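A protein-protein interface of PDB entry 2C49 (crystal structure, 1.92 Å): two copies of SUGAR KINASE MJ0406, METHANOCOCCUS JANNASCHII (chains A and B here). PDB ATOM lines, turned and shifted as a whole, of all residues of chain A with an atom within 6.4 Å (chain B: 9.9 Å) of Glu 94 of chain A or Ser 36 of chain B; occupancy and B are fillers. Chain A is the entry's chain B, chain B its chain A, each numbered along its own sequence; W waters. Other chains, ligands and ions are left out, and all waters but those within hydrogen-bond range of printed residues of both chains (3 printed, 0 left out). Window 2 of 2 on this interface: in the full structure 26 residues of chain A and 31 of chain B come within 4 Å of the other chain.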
ATOM      1  N   VAL A  65      -7.213 -20.968  -9.089  1.00  0.00           N
ATOM      2  CA  VAL A  65      -7.849 -19.658  -9.277  1.00  0.00           C
ATOM      3  C   VAL A  65      -9.237 -19.680  -8.623  1.00  0.00           C
ATOM      4  O   VAL A  65      -9.713 -20.745  -8.235  1.00  0.00           O
ATOM      5  CB  VAL A  65      -7.872 -19.207 -10.773  1.00  0.00           C
ATOM      6  CG1 VAL A  65      -6.433 -19.164 -11.377  1.00  0.00           C
ATOM      7  CG2 VAL A  65      -8.790 -20.101 -11.602  1.00  0.00           C
ATOM      8  N   GLY A  66      -9.866 -18.513  -8.469  1.00  0.00           N
ATOM      9  CA  GLY A  66     -11.096 -18.421  -7.715  1.00  0.00           C
ATOM     10  C   GLY A  66     -12.304 -18.119  -8.588  1.00  0.00           C
ATOM     11  O   GLY A  66     -12.204 -18.064  -9.813  1.00  0.00           O
ATOM     12  N   TYR A  67     -13.427 -17.887  -7.946  1.00  0.00           N
ATOM     13  CA  TYR A  67     -14.697 -17.657  -8.651  1.00  0.00           C
ATOM     14  C   TYR A  67     -14.799 -16.278  -9.333  1.00  0.00           C
ATOM     15  O   TYR A  67     -15.768 -16.007 -10.023  1.00  0.00           O
ATOM     16  CB  TYR A  67     -15.855 -17.888  -7.697  1.00  0.00           C
ATOM     17  CG  TYR A  67     -15.822 -17.050  -6.424  1.00  0.00           C
ATOM     18  CD1 TYR A  67     -16.011 -15.668  -6.463  1.00  0.00           C
ATOM     19  CD2 TYR A  67     -15.617 -17.653  -5.186  1.00  0.00           C
ATOM     20  CE1 TYR A  67     -16.004 -14.908  -5.276  1.00  0.00           C
ATOM     21  CE2 TYR A  67     -15.605 -16.920  -4.000  1.00  0.00           C
ATOM     22  CZ  TYR A  67     -15.800 -15.545  -4.050  1.00  0.00           C
ATOM     23  OH  TYR A  67     -15.786 -14.830  -2.881  1.00  0.00           O
ATOM     24  N   ASP A  68     -13.784 -15.431  -9.146  1.00  0.00           N
ATOM     25  CA  ASP A  68     -13.708 -14.133  -9.800  1.00  0.00           C
ATOM     26  C   ASP A  68     -12.717 -14.158 -10.961  1.00  0.00           C
ATOM     27  O   ASP A  68     -12.506 -13.154 -11.623  1.00  0.00           O
ATOM     28  CB  ASP A  68     -13.283 -13.036  -8.797  1.00  0.00           C
ATOM     29  CG  ASP A  68     -11.918 -13.340  -8.146  1.00  0.00           C
ATOM     30  OD1 ASP A  68     -11.571 -14.524  -8.036  1.00  0.00           O
ATOM     31  OD2 ASP A  68     -11.144 -12.472  -7.712  1.00  0.00           O
ATOM     32  N   LYS A  70     -12.895 -15.530 -13.629  1.00  0.00           N
ATOM     33  CA  LYS A  70     -13.426 -16.816 -14.093  1.00  0.00           C
ATOM     34  C   LYS A  70     -14.244 -16.768 -15.378  1.00  0.00           C
ATOM     35  O   LYS A  70     -14.462 -17.808 -16.027  1.00  0.00           O
ATOM     36  CB  LYS A  70     -14.348 -17.317 -12.972  1.00  0.00           C
ATOM     37  CG  LYS A  70     -13.995 -18.630 -12.318  1.00  0.00           C
ATOM     38  CD  LYS A  70     -15.273 -19.427 -11.898  1.00  0.00           C
ATOM     39  CE  LYS A  70     -14.926 -20.757 -11.194  1.00  0.00           C
ATOM     40  NZ  LYS A  70     -15.363 -20.891  -9.748  1.00  0.00           N
ATOM     41  N   SER A  91     -11.719 -22.624  -7.910  1.00  0.00           N
ATOM     42  CA  SER A  91     -12.458 -22.720  -6.659  1.00  0.00           C
ATOM     43  C   SER A  91     -13.844 -22.116  -6.778  1.00  0.00           C
ATOM     44  O   SER A  91     -14.028 -21.024  -7.316  1.00  0.00           O
ATOM     45  CB  SER A  91     -11.711 -22.004  -5.528  1.00  0.00           C
ATOM     46  OG  SER A  91     -12.494 -21.954  -4.338  1.00  0.00           O
ATOM     47  N   GLU A  92     -14.816 -22.833  -6.226  1.00  0.00           N
ATOM     48  CA  GLU A  92     -16.083 -22.257  -5.893  1.00  0.00           C
ATOM     49  C   GLU A  92     -16.035 -21.563  -4.513  1.00  0.00           C
ATOM     50  O   GLU A  92     -17.031 -20.904  -4.125  1.00  0.00           O
ATOM     51  CB  GLU A  92     -17.146 -23.354  -5.926  1.00  0.00           C
ATOM     52  CG  GLU A  92     -17.315 -23.924  -7.336  1.00  0.00           C
ATOM     53  CD  GLU A  92     -18.071 -25.242  -7.314  1.00  0.00           C
ATOM     54  OE1 GLU A  92     -17.436 -26.287  -7.010  1.00  0.00           O
ATOM     55  OE2 GLU A  92     -19.296 -25.217  -7.560  1.00  0.00           O
ATOM     56  N   GLU A  93     -15.028 -21.755  -3.688  1.00  0.00           N
ATOM     57  CA  GLU A  93     -15.233 -21.209  -2.359  1.00  0.00           C
ATOM     58  C   GLU A  93     -14.478 -19.941  -2.079  1.00  0.00           C
ATOM     59  O   GLU A  93     -14.776 -19.215  -1.138  1.00  0.00           O
ATOM     60  CB  GLU A  93     -14.896 -22.316  -1.350  1.00  0.00           C
ATOM     61  CG  GLU A  93     -14.958 -23.746  -1.861  1.00  0.00           C
ATOM     62  CD  GLU A  93     -14.881 -24.786  -0.739  1.00  0.00           C
ATOM     63  OE1 GLU A  93     -15.697 -25.721  -0.755  1.00  0.00           O
ATOM     64  OE2 GLU A  93     -13.998 -24.644   0.138  1.00  0.00           O
ATOM     65  N   GLU A  94     -13.485 -19.666  -2.919  1.00  0.00           N
ATOM     66  CA  GLU A  94     -12.478 -18.597  -2.636  1.00  0.00           C
ATOM     67  C   GLU A  94     -12.153 -17.778  -3.878  1.00  0.00           C
ATOM     68  O   GLU A  94     -12.236 -18.277  -5.003  1.00  0.00           O
ATOM     69  CB  GLU A  94     -11.161 -19.217  -2.119  1.00  0.00           C
ATOM     70  CG  GLU A  94     -11.368 -20.174  -0.943  1.00  0.00           C
ATOM     71  CD  GLU A  94     -11.696 -19.467   0.362  1.00  0.00           C
ATOM     72  OE1 GLU A  94     -11.563 -18.210   0.460  1.00  0.00           O
ATOM     73  OE2 GLU A  94     -12.132 -20.175   1.289  1.00  0.00           O
ATOM     74  N   GLU A  95     -11.740 -16.529  -3.665  1.00  0.00           N
ATOM     75  CA  GLU A  95     -11.297 -15.657  -4.753  1.00  0.00           C
ATOM     76  C   GLU A  95      -9.931 -16.105  -5.230  1.00  0.00           C
ATOM     77  O   GLU A  95      -9.222 -16.837  -4.525  1.00  0.00           O
ATOM     78  CB  GLU A  95     -11.255 -14.157  -4.322  1.00  0.00           C
ATOM     79  CG  GLU A  95     -12.599 -13.563  -3.866  1.00  0.00           C
ATOM     80  CD  GLU A  95     -12.576 -12.033  -3.713  1.00  0.00           C
ATOM     81  OE1 GLU A  95     -13.650 -11.436  -3.526  1.00  0.00           O
ATOM     82  OE2 GLU A  95     -11.481 -11.411  -3.766  1.00  0.00           O
ATOM     83  N   THR A  96      -9.590 -15.689  -6.448  1.00  0.00           N
ATOM     84  CA  THR A  96      -8.237 -15.816  -7.012  1.00  0.00           C
ATOM     85  C   THR A  96      -7.221 -15.137  -6.057  1.00  0.00           C
ATOM     86  O   THR A  96      -7.516 -14.058  -5.526  1.00  0.00           O
ATOM     87  CB  THR A  96      -8.252 -15.158  -8.399  1.00  0.00           C
ATOM     88  OG1 THR A  96      -9.248 -15.823  -9.219  1.00  0.00           O
ATOM     89  CG2 THR A  96      -6.926 -15.351  -9.171  1.00  0.00           C
ATOM     90  N   LEU A 114      -3.734 -12.193  -0.438  1.00  0.00           N
ATOM     91  CA  LEU A 114      -4.868 -13.081  -0.242  1.00  0.00           C
ATOM     92  C   LEU A 114      -4.425 -14.456  -0.715  1.00  0.00           C
ATOM     93  O   LEU A 114      -4.081 -14.643  -1.889  1.00  0.00           O
ATOM     94  CB  LEU A 114      -6.111 -12.568  -0.992  1.00  0.00           C
ATOM     95  CG  LEU A 114      -7.327 -13.507  -0.989  1.00  0.00           C
ATOM     96  CD1 LEU A 114      -7.780 -13.862   0.467  1.00  0.00           C
ATOM     97  CD2 LEU A 114      -8.493 -12.935  -1.843  1.00  0.00           C
ATOM     98  N   TRP A 115      -4.444 -15.426   0.212  1.00  0.00           N
ATOM     99  CA  TRP A 115      -4.175 -16.830  -0.142  1.00  0.00           C
ATOM    100  C   TRP A 115      -5.321 -17.414  -0.999  1.00  0.00           C
ATOM    101  O   TRP A 115      -5.066 -17.984  -2.070  1.00  0.00           O
ATOM    102  CB  TRP A 115      -3.965 -17.644   1.151  1.00  0.00           C
ATOM    103  CG  TRP A 115      -3.574 -19.112   1.005  1.00  0.00           C
ATOM    104  CD1 TRP A 115      -4.255 -20.184   1.525  1.00  0.00           C
ATOM    105  CD2 TRP A 115      -2.379 -19.664   0.402  1.00  0.00           C
ATOM    106  NE1 TRP A 115      -3.585 -21.351   1.252  1.00  0.00           N
ATOM    107  CE2 TRP A 115      -2.446 -21.066   0.544  1.00  0.00           C
ATOM    108  CE3 TRP A 115      -1.267 -19.116  -0.266  1.00  0.00           C
ATOM    109  CZ2 TRP A 115      -1.427 -21.933   0.080  1.00  0.00           C
ATOM    110  CZ3 TRP A 115      -0.279 -19.975  -0.735  1.00  0.00           C
ATOM    111  CH2 TRP A 115      -0.374 -21.371  -0.565  1.00  0.00           C
ATOM    112  N   GLY A 116      -6.561 -17.256  -0.514  1.00  0.00           N
ATOM    113  CA  GLY A 116      -7.776 -17.561  -1.264  1.00  0.00           C
ATOM    114  C   GLY A 116      -7.801 -18.948  -1.874  1.00  0.00           C
ATOM    115  O   GLY A 116      -7.715 -19.939  -1.131  1.00  0.00           O
ATOM    116  N   ALA A 117      -7.907 -19.030  -3.207  1.00  0.00           N
ATOM    117  CA  ALA A 117      -8.029 -20.322  -3.860  1.00  0.00           C
ATOM    118  C   ALA A 117      -6.781 -21.218  -3.670  1.00  0.00           C
ATOM    119  O   ALA A 117      -6.861 -22.453  -3.826  1.00  0.00           O
ATOM    120  CB  ALA A 117      -8.364 -20.159  -5.351  1.00  0.00           C
ATOM    121  N   ALA A 118      -5.635 -20.628  -3.338  1.00  0.00           N
ATOM    122  CA  ALA A 118      -4.462 -21.464  -3.092  1.00  0.00           C
ATOM    123  C   ALA A 118      -4.659 -22.489  -1.964  1.00  0.00           C
ATOM    124  O   ALA A 118      -3.834 -23.393  -1.804  1.00  0.00           O
ATOM    125  CB  ALA A 118      -3.215 -20.656  -2.876  1.00  0.00           C
ATOM    126  N   LYS A 119      -5.718 -22.343  -1.175  1.00  0.00           N
ATOM    127  CA  LYS A 119      -6.032 -23.358  -0.176  1.00  0.00           C
ATOM    128  C   LYS A 119      -6.275 -24.721  -0.836  1.00  0.00           C
ATOM    129  O   LYS A 119      -6.201 -25.744  -0.174  1.00  0.00           O
ATOM    130  CB  LYS A 119      -7.227 -22.954   0.706  1.00  0.00           C
ATOM    131  CG  LYS A 119      -8.596 -23.201   0.070  1.00  0.00           C
ATOM    132  CD  LYS A 119      -9.757 -22.935   1.068  1.00  0.00           C
ATOM    133  CE  LYS A 119     -11.080 -23.413   0.508  1.00  0.00           C
ATOM    134  NZ  LYS A 119     -12.305 -22.834   1.231  1.00  0.00           N
ATOM    135  N   HIS A 120      -6.600 -24.732  -2.120  1.00  0.00           N
ATOM    136  CA  HIS A 120      -6.938 -26.000  -2.770  1.00  0.00           C
ATOM    137  C   HIS A 120      -5.763 -26.918  -3.107  1.00  0.00           C
ATOM    138  O   HIS A 120      -5.970 -28.129  -3.280  1.00  0.00           O
ATOM    139  CB  HIS A 120      -7.858 -25.805  -3.978  1.00  0.00           C
ATOM    140  CG  HIS A 120      -9.215 -25.268  -3.622  1.00  0.00           C
ATOM    141  ND1 HIS A 120     -10.187 -26.037  -3.028  1.00  0.00           N
ATOM    142  CD2 HIS A 120      -9.740 -24.021  -3.734  1.00  0.00           C
ATOM    143  CE1 HIS A 120     -11.274 -25.306  -2.833  1.00  0.00           C
ATOM    144  NE2 HIS A 120     -11.026 -24.076  -3.250  1.00  0.00           N
ATOM    145  N   ASP B  17     -17.254  -4.163   0.154  1.00  0.00           N
ATOM    146  CA  ASP B  17     -16.356  -4.140   1.285  1.00  0.00           C
ATOM    147  C   ASP B  17     -15.621  -5.464   1.402  1.00  0.00           C
ATOM    148  O   ASP B  17     -16.251  -6.538   1.300  1.00  0.00           O
ATOM    149  CB  ASP B  17     -17.183  -4.074   2.568  1.00  0.00           C
ATOM    150  CG  ASP B  17     -17.765  -2.717   2.845  1.00  0.00           C
ATOM    151  OD1 ASP B  17     -17.508  -1.711   2.112  1.00  0.00           O
ATOM    152  OD2 ASP B  17     -18.481  -2.560   3.862  1.00  0.00           O
ATOM    153  N   TYR B  18     -14.328  -5.371   1.655  1.00  0.00           N
ATOM    154  CA  TYR B  18     -13.530  -6.467   2.183  1.00  0.00           C
ATOM    155  C   TYR B  18     -13.294  -6.109   3.651  1.00  0.00           C
ATOM    156  O   TYR B  18     -12.983  -4.947   3.963  1.00  0.00           O
ATOM    157  CB  TYR B  18     -12.164  -6.475   1.486  1.00  0.00           C
ATOM    158  CG  TYR B  18     -12.101  -7.113   0.118  1.00  0.00           C
ATOM    159  CD1 TYR B  18     -11.909  -6.327  -1.025  1.00  0.00           C
ATOM    160  CD2 TYR B  18     -12.178  -8.505  -0.033  1.00  0.00           C
ATOM    161  CE1 TYR B  18     -11.781  -6.905  -2.279  1.00  0.00           C
ATOM    162  CE2 TYR B  18     -12.074  -9.098  -1.294  1.00  0.00           C
ATOM    163  CZ  TYR B  18     -11.856  -8.290  -2.412  1.00  0.00           C
ATOM    164  OH  TYR B  18     -11.732  -8.856  -3.659  1.00  0.00           O
ATOM    165  N   ILE B  19     -13.481  -7.064   4.559  1.00  0.00           N
ATOM    166  CA  ILE B  19     -13.374  -6.790   6.000  1.00  0.00           C
ATOM    167  C   ILE B  19     -12.426  -7.834   6.618  1.00  0.00           C
ATOM    168  O   ILE B  19     -12.683  -9.040   6.484  1.00  0.00           O
ATOM    169  CB  ILE B  19     -14.778  -6.831   6.661  1.00  0.00           C
ATOM    170  CG1 ILE B  19     -15.781  -5.883   5.937  1.00  0.00           C
ATOM    171  CG2 ILE B  19     -14.697  -6.556   8.154  1.00  0.00           C
ATOM    172  CD1 ILE B  19     -17.222  -6.025   6.402  1.00  0.00           C
ATOM    173  N   PHE B  20     -11.348  -7.380   7.261  1.00  0.00           N
ATOM    174  CA  PHE B  20     -10.306  -8.274   7.773  1.00  0.00           C
ATOM    175  C   PHE B  20     -10.039  -8.087   9.278  1.00  0.00           C
ATOM    176  O   PHE B  20     -10.026  -6.957   9.793  1.00  0.00           O
ATOM    177  CB  PHE B  20      -8.955  -8.099   7.047  1.00  0.00           C
ATOM    178  CG  PHE B  20      -9.043  -7.997   5.548  1.00  0.00           C
ATOM    179  CD1 PHE B  20      -9.146  -6.754   4.931  1.00  0.00           C
ATOM    180  CD2 PHE B  20      -8.967  -9.135   4.758  1.00  0.00           C
ATOM    181  CE1 PHE B  20      -9.209  -6.647   3.555  1.00  0.00           C
ATOM    182  CE2 PHE B  20      -9.022  -9.046   3.386  1.00  0.00           C
ATOM    183  CZ  PHE B  20      -9.149  -7.802   2.778  1.00  0.00           C
ATOM    184  N   ASN B  21      -9.833  -9.221   9.952  1.00  0.00           N
ATOM    185  CA  ASN B  21      -9.384  -9.289  11.332  1.00  0.00           C
ATOM    186  C   ASN B  21      -7.892  -9.504  11.354  1.00  0.00           C
ATOM    187  O   ASN B  21      -7.368 -10.425  10.686  1.00  0.00           O
ATOM    188  CB  ASN B  21     -10.046 -10.458  12.045  1.00  0.00           C
ATOM    189  CG  ASN B  21     -11.464 -10.170  12.413  1.00  0.00           C
ATOM    190  OD1 ASN B  21     -11.731  -9.626  13.480  1.00  0.00           O
ATOM    191  ND2 ASN B  21     -12.398 -10.544  11.536  1.00  0.00           N
ATOM    192  N   ILE B  32       1.493  -9.165   4.915  1.00  0.00           N
ATOM    193  CA  ILE B  32       0.645 -10.051   5.681  1.00  0.00           C
ATOM    194  C   ILE B  32      -0.114 -10.935   4.667  1.00  0.00           C
ATOM    195  O   ILE B  32      -0.518 -10.459   3.604  1.00  0.00           O
ATOM    196  CB  ILE B  32      -0.299  -9.184   6.555  1.00  0.00           C
ATOM    197  CG1 ILE B  32       0.436  -8.670   7.804  1.00  0.00           C
ATOM    198  CG2 ILE B  32      -1.576  -9.922   6.964  1.00  0.00           C
ATOM    199  CD1 ILE B  32       0.990  -9.759   8.733  1.00  0.00           C
ATOM    200  N   GLN B  33      -0.259 -12.217   4.974  1.00  0.00           N
ATOM    201  CA  GLN B  33      -1.131 -13.083   4.177  1.00  0.00           C
ATOM    202  C   GLN B  33      -2.488 -13.215   4.835  1.00  0.00           C
ATOM    203  O   GLN B  33      -2.586 -13.494   6.036  1.00  0.00           O
ATOM    204  CB  GLN B  33      -0.522 -14.485   3.975  1.00  0.00           C
ATOM    205  CG  GLN B  33      -1.205 -15.292   2.827  1.00  0.00           C
ATOM    206  CD  GLN B  33      -0.341 -16.449   2.365  1.00  0.00           C
ATOM    207  OE1 GLN B  33       0.620 -16.251   1.583  1.00  0.00           O
ATOM    208  NE2 GLN B  33      -0.653 -17.666   2.856  1.00  0.00           N
ATOM    209  N   ILE B  34      -3.532 -13.042   4.030  1.00  0.00           N
ATOM    210  CA  ILE B  34      -4.897 -13.235   4.455  1.00  0.00           C
ATOM    211  C   ILE B  34      -5.380 -14.607   3.934  1.00  0.00           C
ATOM    212  O   ILE B  34      -5.485 -14.798   2.741  1.00  0.00           O
ATOM    213  CB  ILE B  34      -5.793 -12.085   3.881  1.00  0.00           C
ATOM    214  CG1 ILE B  34      -5.339 -10.696   4.383  1.00  0.00           C
ATOM    215  CG2 ILE B  34      -7.303 -12.365   4.134  1.00  0.00           C
ATOM    216  CD1 ILE B  34      -5.304 -10.547   5.922  1.00  0.00           C
ATOM    217  N   PRO B  35      -5.691 -15.559   4.813  1.00  0.00           N
ATOM    218  CA  PRO B  35      -6.173 -16.873   4.354  1.00  0.00           C
ATOM    219  C   PRO B  35      -7.364 -16.764   3.369  1.00  0.00           C
ATOM    220  O   PRO B  35      -7.295 -17.364   2.304  1.00  0.00           O
ATOM    221  CB  PRO B  35      -6.584 -17.561   5.656  1.00  0.00           C
ATOM    222  CG  PRO B  35      -5.573 -16.968   6.672  1.00  0.00           C
ATOM    223  CD  PRO B  35      -5.597 -15.484   6.281  1.00  0.00           C
ATOM    224  N   SER B  36      -8.386 -15.978   3.701  1.00  0.00           N
ATOM    225  CA  SER B  36      -9.654 -16.020   2.979  1.00  0.00           C
ATOM    226  C   SER B  36     -10.374 -14.675   3.024  1.00  0.00           C
ATOM    227  O   SER B  36     -10.444 -14.030   4.085  1.00  0.00           O
ATOM    228  CB  SER B  36     -10.536 -17.165   3.531  1.00  0.00           C
ATOM    229  OG  SER B  36     -11.864 -17.165   2.992  1.00  0.00           O
ATOM    230  N   ALA B  37     -10.894 -14.233   1.875  1.00  0.00           N
ATOM    231  CA  ALA B  37     -11.676 -13.007   1.828  1.00  0.00           C
ATOM    232  C   ALA B  37     -12.837 -13.095   0.875  1.00  0.00           C
ATOM    233  O   ALA B  37     -12.801 -13.822  -0.140  1.00  0.00           O
ATOM    234  CB  ALA B  37     -10.805 -11.765   1.512  1.00  0.00           C
ATOM    235  N   ARG B  38     -13.835 -12.312   1.229  1.00  0.00           N
ATOM    236  CA  ARG B  38     -15.115 -12.266   0.604  1.00  0.00           C
ATOM    237  C   ARG B  38     -15.553 -10.803   0.533  1.00  0.00           C
ATOM    238  O   ARG B  38     -15.227 -10.037   1.427  1.00  0.00           O
ATOM    239  CB  ARG B  38     -16.113 -12.924   1.546  1.00  0.00           C
ATOM    240  CG  ARG B  38     -16.968 -14.044   1.002  1.00  0.00           C
ATOM    241  CD  ARG B  38     -18.237 -14.079   1.842  1.00  0.00           C
ATOM    242  NE  ARG B  38     -19.075 -12.929   1.576  1.00  0.00           N
ATOM    243  CZ  ARG B  38     -20.378 -13.020   1.378  1.00  0.00           C
ATOM    244  NH1 ARG B  38     -20.986 -14.196   1.431  1.00  0.00           N
ATOM    245  NH2 ARG B  38     -21.089 -11.919   1.141  1.00  0.00           N
ATOM    246  N   LYS B  39     -16.262 -10.405  -0.510  1.00  0.00           N
ATOM    247  CA  LYS B  39     -16.758  -9.028  -0.561  1.00  0.00           C
ATOM    248  C   LYS B  39     -18.134  -9.005   0.033  1.00  0.00           C
ATOM    249  O   LYS B  39     -18.904  -9.953  -0.146  1.00  0.00           O
ATOM    250  CB  LYS B  39     -16.858  -8.492  -1.987  1.00  0.00           C
ATOM    251  CG  LYS B  39     -15.544  -8.426  -2.788  1.00  0.00           C
ATOM    252  CD  LYS B  39     -15.827  -8.021  -4.238  1.00  0.00           C
ATOM    253  CE  LYS B  39     -14.548  -8.069  -5.106  1.00  0.00           C
ATOM    254  NZ  LYS B  39     -14.095  -9.509  -5.354  1.00  0.00           N
ATOM    255  N   TYR B  40     -18.439  -7.923   0.745  1.00  0.00           N
ATOM    256  CA  TYR B  40     -19.757  -7.727   1.362  1.00  0.00           C
ATOM    257  C   TYR B  40     -20.409  -6.470   0.822  1.00  0.00           C
ATOM    258  O   TYR B  40     -19.708  -5.502   0.501  1.00  0.00           O
ATOM    259  CB  TYR B  40     -19.586  -7.565   2.861  1.00  0.00           C
ATOM    260  CG  TYR B  40     -19.004  -8.792   3.506  1.00  0.00           C
ATOM    261  CD1 TYR B  40     -17.611  -8.977   3.579  1.00  0.00           C
ATOM    262  CD2 TYR B  40     -19.830  -9.778   4.006  1.00  0.00           C
ATOM    263  CE1 TYR B  40     -17.078 -10.112   4.190  1.00  0.00           C
ATOM    264  CE2 TYR B  40     -19.294 -10.933   4.611  1.00  0.00           C
ATOM    265  CZ  TYR B  40     -17.923 -11.081   4.690  1.00  0.00           C
ATOM    266  OH  TYR B  40     -17.397 -12.199   5.275  1.00  0.00           O
ATOM    267  N   ILE B 101     -11.205  -2.882   4.938  1.00  0.00           N
ATOM    268  CA  ILE B 101     -11.446  -2.553   6.340  1.00  0.00           C
ATOM    269  C   ILE B 101     -10.719  -3.546   7.231  1.00  0.00           C
ATOM    270  O   ILE B 101     -10.901  -4.768   7.102  1.00  0.00           O
ATOM    271  CB  ILE B 101     -12.976  -2.579   6.605  1.00  0.00           C
ATOM    272  CG1 ILE B 101     -13.669  -1.545   5.690  1.00  0.00           C
ATOM    273  CG2 ILE B 101     -13.296  -2.335   8.096  1.00  0.00           C
ATOM    274  CD1 ILE B 101     -15.170  -1.717   5.550  1.00  0.00           C
ATOM    275  N   PHE B 102      -9.867  -3.011   8.103  1.00  0.00           N
ATOM    276  CA  PHE B 102      -9.057  -3.839   8.983  1.00  0.00           C
ATOM    277  C   PHE B 102      -9.447  -3.561  10.400  1.00  0.00           C
ATOM    278  O   PHE B 102      -9.552  -2.416  10.785  1.00  0.00           O
ATOM    279  CB  PHE B 102      -7.569  -3.578   8.761  1.00  0.00           C
ATOM    280  CG  PHE B 102      -7.147  -3.857   7.372  1.00  0.00           C
ATOM    281  CD1 PHE B 102      -7.347  -2.919   6.376  1.00  0.00           C
ATOM    282  CD2 PHE B 102      -6.589  -5.078   7.045  1.00  0.00           C
ATOM    283  CE1 PHE B 102      -6.986  -3.203   5.064  1.00  0.00           C
ATOM    284  CE2 PHE B 102      -6.230  -5.351   5.744  1.00  0.00           C
ATOM    285  CZ  PHE B 102      -6.423  -4.410   4.763  1.00  0.00           C
ATOM    286  N   LYS B 281     -20.203 -10.815  10.279  1.00  0.00           N
ATOM    287  CA  LYS B 281     -19.356  -9.974   9.425  1.00  0.00           C
ATOM    288  C   LYS B 281     -20.168  -9.475   8.234  1.00  0.00           C
ATOM    289  O   LYS B 281     -20.970 -10.209   7.664  1.00  0.00           O
ATOM    290  CB  LYS B 281     -18.106 -10.736   8.940  1.00  0.00           C
ATOM    291  CG  LYS B 281     -17.060  -9.889   8.228  1.00  0.00           C
ATOM    292  CD  LYS B 281     -15.761 -10.711   8.026  1.00  0.00           C
ATOM    293  CE  LYS B 281     -14.686 -10.289   9.026  1.00  0.00           C
ATOM    294  NZ  LYS B 281     -13.408 -10.935   8.681  1.00  0.00           N
HETATM  295  O   HOH W   1     -11.162 -15.796  -0.713  1.00  0.00           O
HETATM  296  O   HOH W   2      -8.231 -19.869   1.636  1.00  0.00           O
HETATM  297  O   HOH W   3     -15.965 -12.149  -2.949  1.00  0.00           O
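The side-chain hydroxyl (OH) of Tyr 18 of chain B is in hydrogen-bond range of the side-chain carboxylate (OE2) of Glu 95 of chain A (2.6 Å). OE1 of Glu 95 of chain A lies within salt-bridge range of NZ of Lys 39 of chain B (2.7 Å). N of Gly 116 of chain A lies within hydrogen-bond range of O of Pro 35 of chain B, at 2.9 Å. The backbone NH (N) of Trp 115 of chain A sits at hydrogen-bond distance from the backbone carbonyl oxygen (O) of Ile 34 of chain B (2.8 Å). The side-chain hydroxyl (OG) of Ser 36 of chain B lies within hydrogen-bond range of the side-chain carboxylate (OE1) of Glu 94 of chain A, 2.8 Å away.
N of Ala 117 of chain A sits at hydrogen-bond distance from O of Glu 95 of chain A. The side-chain carboxylate (OE2) of Glu 94 of chain A lies within salt-bridge range of the side-chain amino group (NZ) of Lys 119 of chain A, at 2.7 Å. N of Ile 101 of chain B lies within hydrogen-bond range of O of Tyr 18 of chain B (2.9 Å). The side-chain hydroxyl (OH) of Tyr 18 of chain B sits at hydrogen-bond distance from the side-chain amino group (NZ) of Lys 39 of chain B, 3.0 Å away. The backbone carbonyl oxygen (O) of Glu 94 of chain A sits at hydrogen-bond distance from the backbone NH (N) of Tyr 67 of chain A (3.2 Å).
Among the printed residues, pairs that only touch across the chains: Leu 114 of chain A with Ile 34 of chain B (3.4 Å), Leu 114 of chain A with Ala 37 of chain B (3.4 Å), Trp 115 of chain A with Gln 33 of chain B (3.5 Å), Trp 115 of chain A with Pro 35 of chain B (3.5 Å), Leu 114 of chain A with Ser 36 of chain B (3.7 Å), Glu 95 of chain A with Ala 37 of chain B (3.7 Å) and Leu 114 of chain A with Pro 35 of chain B (3.98 Å).
No residue of chain B comes within 4 Å of Gly 66 of chain A. No residue of chain B comes within 4 Å of Ser 91 of chain A. Printed residues of chain B within 4 Å of Glu 95 of chain A: Tyr 18 (2.6 Å), Ala 37 (3.7 Å) and Lys 39 (2.7 Å). Of the printed residues of chain B, Trp 115 of chain A touches Gln 33, Ile 34 and Pro 35. No residue of chain B comes within 4 Å of Ala 117 of chain A. Ile 32 of chain B touches none of the printed residues of chain A. Printed residues of chain A within 4 Å of Ser 36 of chain B: Glu 94 (2.8 Å) and Leu 114 (3.7 Å). Of the printed residues of chain A, Lys 39 of chain B touches Glu 95 (2.7 Å). The nearest residue of chain B that does not touch Glu 94 of chain A is Ala 37 of chain B (4.3 Å). The nearest residue of chain A that does not touch Ser 36 of chain B is Gly 116 of chain A (4.8 Å).
Of the 17 printed residues of chain B, 7 touch a printed residue of chain A. Hydrophobic or aromatic side chains of chain B that line the printed part of chain A: Tyr 18, Ile 34 and Ala 37. Along chain B the printed residues that touch a printed residue of chain A span positions 18 to 39. Of the 18 printed residues of chain A, 5 touch a printed residue of chain B. Hydrophobic or aromatic side chains of chain A that line the printed part of chain B: Leu 114 and Trp 115. Along chain A the printed residues that touch a printed residue of chain B span positions 94 to 116. Among the printed residues, Asp or Glu carboxylates within 4 Å of a Lys or Arg side-chain nitrogen of the other chain: Glu 95 of chain A with Lys 39 of chain B (2.7 Å).
No position is printed for both chains.
Water W3 lies within hydrogen-bond range of the side-chain carboxylate of Glu 95 of chain A (2.5 Å), the side-chain hydroxyl of Tyr 67 of chain A (2.7 Å) and the backbone NH of Lys 39 of chain B (3.0 Å). Water W1 lies within hydrogen-bond range of the backbone carbonyl oxygen (O) of Ala 37 of chain B (2.6 Å), the side-chain carboxylate (OE1) of Glu 94 of chain A (2.7 Å) and the backbone NH (N) of Glu 95 of chain A (3.1 Å). Water W2 bridges the backbone carbonyl oxygen (O) of Pro 35 of chain B and the backbone carbonyl oxygen (O) of Gly 116 of chain A.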
